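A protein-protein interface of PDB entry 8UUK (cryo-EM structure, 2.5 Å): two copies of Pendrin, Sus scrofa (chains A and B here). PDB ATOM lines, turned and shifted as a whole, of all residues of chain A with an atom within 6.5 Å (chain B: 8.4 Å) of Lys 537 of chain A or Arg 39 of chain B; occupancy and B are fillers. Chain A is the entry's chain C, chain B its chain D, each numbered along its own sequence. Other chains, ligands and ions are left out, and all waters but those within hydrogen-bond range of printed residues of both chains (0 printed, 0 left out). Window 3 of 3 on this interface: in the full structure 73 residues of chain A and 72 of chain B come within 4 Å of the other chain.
OD2 of Asp 535 of chain A lies within salt-bridge range of NH2 of Arg 38 of chain B, 3.0 Å away. N of Arg 39 of chain B lies within hydrogen-bond range of O of Asp 535 of chain A (2.5 Å). The side-chain amide oxygen (OE1) of Gln 33 of chain B is in hydrogen-bond range of the side-chain hydroxyl (OH) of Tyr 536 of chain A. O of Glu 37 of chain B lies close to O of Tyr 536 of chain A.
The side-chain carboxylate of Asp 535 of chain A sits close to the side-chain hydroxyl of Ser 532 of chain A, at 3.2 Å. NZ of Lys 534 of chain A is in salt-bridge range of OD1 of Asp 535 of chain A, 3.3 Å away. NH1 of Arg 38 of chain B lies within salt-bridge range of OE2 of Glu 701 of chain B (2.4 Å).
CG of Arg 38 of chain B touches CE2 of Tyr 536 of chain A, 3.7 Å away. Lys 537 of chain A touches Arg 39 of chain B. Asn 538 of chain A touches Tyr 36 of chain B.
Lys 537 of chain A touches just one residue of chain B: Arg 39. Arg 39 of chain B touches just these residues of chain A: Asp 535 (2.5 Å) and Lys 537 (3.3 Å). Of the printed residues of chain A, Arg 38 of chain B touches Asp 535 and Tyr 536. Printed residues of chain B within 4 Å of Asn 538 of chain A: Tyr 36. Of the printed residues of chain A, Tyr 36 of chain B touches Asn 538. Glu 701 of chain B touches none of the printed residues of chain A. Ile 539 of chain A touches none of the printed residues of chain B. The nearest residue of chain B that does not touch Lys 537 of chain A is Glu 37 of chain B (4.9 Å). The nearest residue of chain A that does not touch Arg 39 of chain B is Lys 534 of chain A (4.1 Å).
Of the 7 printed residues of chain B, 5 touch a printed residue of chain A. Of the 8 printed residues of chain A, 4 touch a printed residue of chain B. Printed residues of chain A that touch a printed residue of chain B: Asp 535, Tyr 536, Lys 537 and Asn 538. Hydrophobic or aromatic side chains of chain A that line the printed part of chain B: Tyr 536.
No position is printed for both chains. Of the 7 pairs that touch across the chains among the printed residues, none has its exchanged pair printed and touching as well.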
ATOM      1  N   SER A 532      19.452   4.870 -28.749  1.00  0.00           N
ATOM      2  CA  SER A 532      19.369   4.823 -27.295  1.00  0.00           C
ATOM      3  C   SER A 532      20.105   3.603 -26.754  1.00  0.00           C
ATOM      4  O   SER A 532      19.968   2.493 -27.277  1.00  0.00           O
ATOM      5  CB  SER A 532      17.909   4.807 -26.851  1.00  0.00           C
ATOM      6  OG  SER A 532      17.132   3.981 -27.694  1.00  0.00           O
ATOM      7  N   THR A 533      20.895   3.819 -25.700  1.00  0.00           N
ATOM      8  CA  THR A 533      21.725   2.758 -25.145  1.00  0.00           C
ATOM      9  C   THR A 533      20.908   1.647 -24.499  1.00  0.00           C
ATOM     10  O   THR A 533      21.394   0.515 -24.404  1.00  0.00           O
ATOM     11  CB  THR A 533      22.701   3.337 -24.120  1.00  0.00           C
ATOM     12  OG1 THR A 533      21.967   3.849 -23.000  1.00  0.00           O
ATOM     13  CG2 THR A 533      23.513   4.461 -24.736  1.00  0.00           C
ATOM     14  N   LYS A 534      19.692   1.940 -24.051  1.00  0.00           N
ATOM     15  CA  LYS A 534      18.870   0.966 -23.347  1.00  0.00           C
ATOM     16  C   LYS A 534      17.932   0.198 -24.266  1.00  0.00           C
ATOM     17  O   LYS A 534      17.137  -0.610 -23.776  1.00  0.00           O
ATOM     18  CB  LYS A 534      18.051   1.660 -22.255  1.00  0.00           C
ATOM     19  CG  LYS A 534      17.127   2.748 -22.775  1.00  0.00           C
ATOM     20  CD  LYS A 534      16.290   3.346 -21.658  1.00  0.00           C
ATOM     21  CE  LYS A 534      15.458   4.514 -22.163  1.00  0.00           C
ATOM     22  NZ  LYS A 534      14.534   4.101 -23.255  1.00  0.00           N
ATOM     23  N   ASP A 535      17.999   0.422 -25.576  1.00  0.00           N
ATOM     24  CA  ASP A 535      17.050  -0.175 -26.505  1.00  0.00           C
ATOM     25  C   ASP A 535      17.648  -1.226 -27.425  1.00  0.00           C
ATOM     26  O   ASP A 535      16.908  -2.080 -27.914  1.00  0.00           O
ATOM     27  CB  ASP A 535      16.395   0.909 -27.368  1.00  0.00           C
ATOM     28  CG  ASP A 535      15.308   1.664 -26.631  1.00  0.00           C
ATOM     29  OD1 ASP A 535      15.302   1.631 -25.383  1.00  0.00           O
ATOM     30  OD2 ASP A 535      14.461   2.292 -27.300  1.00  0.00           O
ATOM     31  N   TYR A 536      18.957  -1.194 -27.681  1.00  0.00           N
ATOM     32  CA  TYR A 536      19.546  -2.078 -28.676  1.00  0.00           C
ATOM     33  C   TYR A 536      20.534  -3.091 -28.116  1.00  0.00           C
ATOM     34  O   TYR A 536      20.788  -4.103 -28.777  1.00  0.00           O
ATOM     35  CB  TYR A 536      20.234  -1.253 -29.772  1.00  0.00           C
ATOM     36  CG  TYR A 536      19.253  -0.599 -30.717  1.00  0.00           C
ATOM     37  CD1 TYR A 536      18.570   0.553 -30.351  1.00  0.00           C
ATOM     38  CD2 TYR A 536      18.993  -1.144 -31.965  1.00  0.00           C
ATOM     39  CE1 TYR A 536      17.666   1.148 -31.205  1.00  0.00           C
ATOM     40  CE2 TYR A 536      18.092  -0.554 -32.827  1.00  0.00           C
ATOM     41  CZ  TYR A 536      17.432   0.591 -32.441  1.00  0.00           C
ATOM     42  OH  TYR A 536      16.532   1.181 -33.297  1.00  0.00           O
ATOM     43  N   LYS A 537      21.112  -2.840 -26.942  1.00  0.00           N
ATOM     44  CA  LYS A 537      21.986  -3.750 -26.204  1.00  0.00           C
ATOM     45  C   LYS A 537      23.320  -3.999 -26.898  1.00  0.00           C
ATOM     46  O   LYS A 537      24.178  -4.683 -26.328  1.00  0.00           O
ATOM     47  CB  LYS A 537      21.318  -5.104 -25.919  1.00  0.00           C
ATOM     48  CG  LYS A 537      20.002  -5.000 -25.165  1.00  0.00           C
ATOM     49  CD  LYS A 537      20.212  -4.489 -23.749  1.00  0.00           C
ATOM     50  CE  LYS A 537      19.514  -3.155 -23.536  1.00  0.00           C
ATOM     51  NZ  LYS A 537      19.542  -2.735 -22.110  1.00  0.00           N
ATOM     52  N   ASN A 538      23.528  -3.472 -28.103  1.00  0.00           N
ATOM     53  CA  ASN A 538      24.829  -3.491 -28.756  1.00  0.00           C
ATOM     54  C   ASN A 538      25.424  -2.094 -28.847  1.00  0.00           C
ATOM     55  O   ASN A 538      26.355  -1.868 -29.626  1.00  0.00           O
ATOM     56  CB  ASN A 538      24.720  -4.114 -30.149  1.00  0.00           C
ATOM     57  CG  ASN A 538      25.980  -4.854 -30.554  1.00  0.00           C
ATOM     58  OD1 ASN A 538      26.675  -5.423 -29.713  1.00  0.00           O
ATOM     59  ND2 ASN A 538      26.280  -4.849 -31.848  1.00  0.00           N
ATOM     60  N   ILE A 539      24.902  -1.160 -28.065  1.00  0.00           N
ATOM     61  CA  ILE A 539      25.279   0.243 -28.138  1.00  0.00           C
ATOM     62  C   ILE A 539      26.346   0.520 -27.090  1.00  0.00           C
ATOM     63  O   ILE A 539      26.180   0.171 -25.916  1.00  0.00           O
ATOM     64  CB  ILE A 539      24.052   1.143 -27.926  1.00  0.00           C
ATOM     65  CG1 ILE A 539      23.085   1.021 -29.107  1.00  0.00           C
ATOM     66  CG2 ILE A 539      24.474   2.570 -27.707  1.00  0.00           C
ATOM     67  CD1 ILE A 539      23.392   1.949 -30.251  1.00  0.00           C
ATOM     68  N   GLN B  33      16.863  -3.429 -38.319  1.00  0.00           N
ATOM     69  CA  GLN B  33      16.250  -4.259 -37.288  1.00  0.00           C
ATOM     70  C   GLN B  33      16.669  -5.717 -37.416  1.00  0.00           C
ATOM     71  O   GLN B  33      16.833  -6.402 -36.400  1.00  0.00           O
ATOM     72  CB  GLN B  33      14.728  -4.134 -37.347  1.00  0.00           C
ATOM     73  CG  GLN B  33      14.191  -2.790 -36.880  1.00  0.00           C
ATOM     74  CD  GLN B  33      14.875  -2.285 -35.626  1.00  0.00           C
ATOM     75  OE1 GLN B  33      15.429  -1.186 -35.607  1.00  0.00           O
ATOM     76  NE2 GLN B  33      14.831  -3.083 -34.565  1.00  0.00           N
ATOM     77  N   TYR B  36      20.632  -5.489 -36.190  1.00  0.00           N
ATOM     78  CA  TYR B  36      20.797  -5.032 -34.813  1.00  0.00           C
ATOM     79  C   TYR B  36      19.488  -5.250 -34.064  1.00  0.00           C
ATOM     80  O   TYR B  36      18.511  -4.526 -34.283  1.00  0.00           O
ATOM     81  CB  TYR B  36      21.218  -3.565 -34.778  1.00  0.00           C
ATOM     82  CG  TYR B  36      22.571  -3.312 -35.398  1.00  0.00           C
ATOM     83  CD1 TYR B  36      23.734  -3.727 -34.765  1.00  0.00           C
ATOM     84  CD2 TYR B  36      22.686  -2.672 -36.623  1.00  0.00           C
ATOM     85  CE1 TYR B  36      24.973  -3.504 -35.330  1.00  0.00           C
ATOM     86  CE2 TYR B  36      23.921  -2.444 -37.197  1.00  0.00           C
ATOM     87  CZ  TYR B  36      25.061  -2.863 -36.546  1.00  0.00           C
ATOM     88  OH  TYR B  36      26.292  -2.639 -37.112  1.00  0.00           O
ATOM     89  N   GLU B  37      19.467  -6.248 -33.184  1.00  0.00           N
ATOM     90  CA  GLU B  37      18.261  -6.563 -32.433  1.00  0.00           C
ATOM     91  C   GLU B  37      17.976  -5.486 -31.393  1.00  0.00           C
ATOM     92  O   GLU B  37      18.885  -4.933 -30.770  1.00  0.00           O
ATOM     93  CB  GLU B  37      18.375  -7.927 -31.742  1.00  0.00           C
ATOM     94  CG  GLU B  37      19.591  -8.143 -30.832  1.00  0.00           C
ATOM     95  CD  GLU B  37      20.917  -8.156 -31.568  1.00  0.00           C
ATOM     96  OE1 GLU B  37      21.077  -8.986 -32.487  1.00  0.00           O
ATOM     97  OE2 GLU B  37      21.798  -7.342 -31.223  1.00  0.00           O
ATOM     98  N   ARG B  38      16.691  -5.199 -31.205  1.00  0.00           N
ATOM     99  CA  ARG B  38      16.253  -4.196 -30.249  1.00  0.00           C
ATOM    100  C   ARG B  38      16.048  -4.844 -28.879  1.00  0.00           C
ATOM    101  O   ARG B  38      16.442  -5.990 -28.645  1.00  0.00           O
ATOM    102  CB  ARG B  38      14.987  -3.507 -30.751  1.00  0.00           C
ATOM    103  CG  ARG B  38      15.196  -2.061 -31.159  1.00  0.00           C
ATOM    104  CD  ARG B  38      13.874  -1.345 -31.361  1.00  0.00           C
ATOM    105  NE  ARG B  38      13.611  -0.383 -30.297  1.00  0.00           N
ATOM    106  CZ  ARG B  38      12.649   0.528 -30.333  1.00  0.00           C
ATOM    107  NH1 ARG B  38      11.837   0.636 -31.371  1.00  0.00           N
ATOM    108  NH2 ARG B  38      12.499   1.354 -29.302  1.00  0.00           N
ATOM    109  N   ARG B  39      15.431  -4.102 -27.961  1.00  0.00           N
ATOM    110  CA  ARG B  39      15.163  -4.566 -26.599  1.00  0.00           C
ATOM    111  C   ARG B  39      16.439  -5.014 -25.893  1.00  0.00           C
ATOM    112  O   ARG B  39      16.772  -4.516 -24.818  1.00  0.00           O
ATOM    113  CB  ARG B  39      14.138  -5.705 -26.607  1.00  0.00           C
ATOM    114  CG  ARG B  39      12.727  -5.271 -26.969  1.00  0.00           C
ATOM    115  CD  ARG B  39      12.030  -4.611 -25.791  1.00  0.00           C
ATOM    116  NE  ARG B  39      10.672  -4.199 -26.124  1.00  0.00           N
ATOM    117  CZ  ARG B  39       9.852  -3.580 -25.286  1.00  0.00           C
ATOM    118  NH1 ARG B  39      10.220  -3.286 -24.050  1.00  0.00           N
ATOM    119  NH2 ARG B  39       8.632  -3.247 -25.698  1.00  0.00           N
ATOM    120  N   GLU B 701       7.222   2.794 -34.044  1.00  0.00           N
ATOM    121  CA  GLU B 701       6.339   1.973 -33.221  1.00  0.00           C
ATOM    122  C   GLU B 701       4.895   2.447 -33.332  1.00  0.00           C
ATOM    123  O   GLU B 701       3.969   1.633 -33.420  1.00  0.00           O
ATOM    124  CB  GLU B 701       6.788   2.000 -31.759  1.00  0.00           C
ATOM    125  CG  GLU B 701       8.251   1.649 -31.489  1.00  0.00           C
ATOM    126  CD  GLU B 701       8.823   0.595 -32.422  1.00  0.00           C
ATOM    127  OE1 GLU B 701       8.143  -0.415 -32.693  1.00  0.00           O
ATOM    128  OE2 GLU B 701       9.968   0.781 -32.886  1.00  0.00           O
ATOM    129  N   GLU B 704       3.520   1.278 -36.614  1.00  0.00           N
ATOM    130  CA  GLU B 704       3.217  -0.149 -36.654  1.00  0.00           C
ATOM    131  C   GLU B 704       1.994  -0.490 -35.810  1.00  0.00           C
ATOM    132  O   GLU B 704       1.260  -1.426 -36.144  1.00  0.00           O
ATOM    133  CB  GLU B 704       4.430  -0.967 -36.206  1.00  0.00           C
ATOM    134  CG  GLU B 704       4.405  -1.419 -34.759  1.00  0.00           C
ATOM    135  CD  GLU B 704       5.784  -1.732 -34.223  1.00  0.00           C
ATOM    136  OE1 GLU B 704       6.747  -1.727 -35.019  1.00  0.00           O
ATOM    137  OE2 GLU B 704       5.903  -1.992 -33.008  1.00  0.00           O
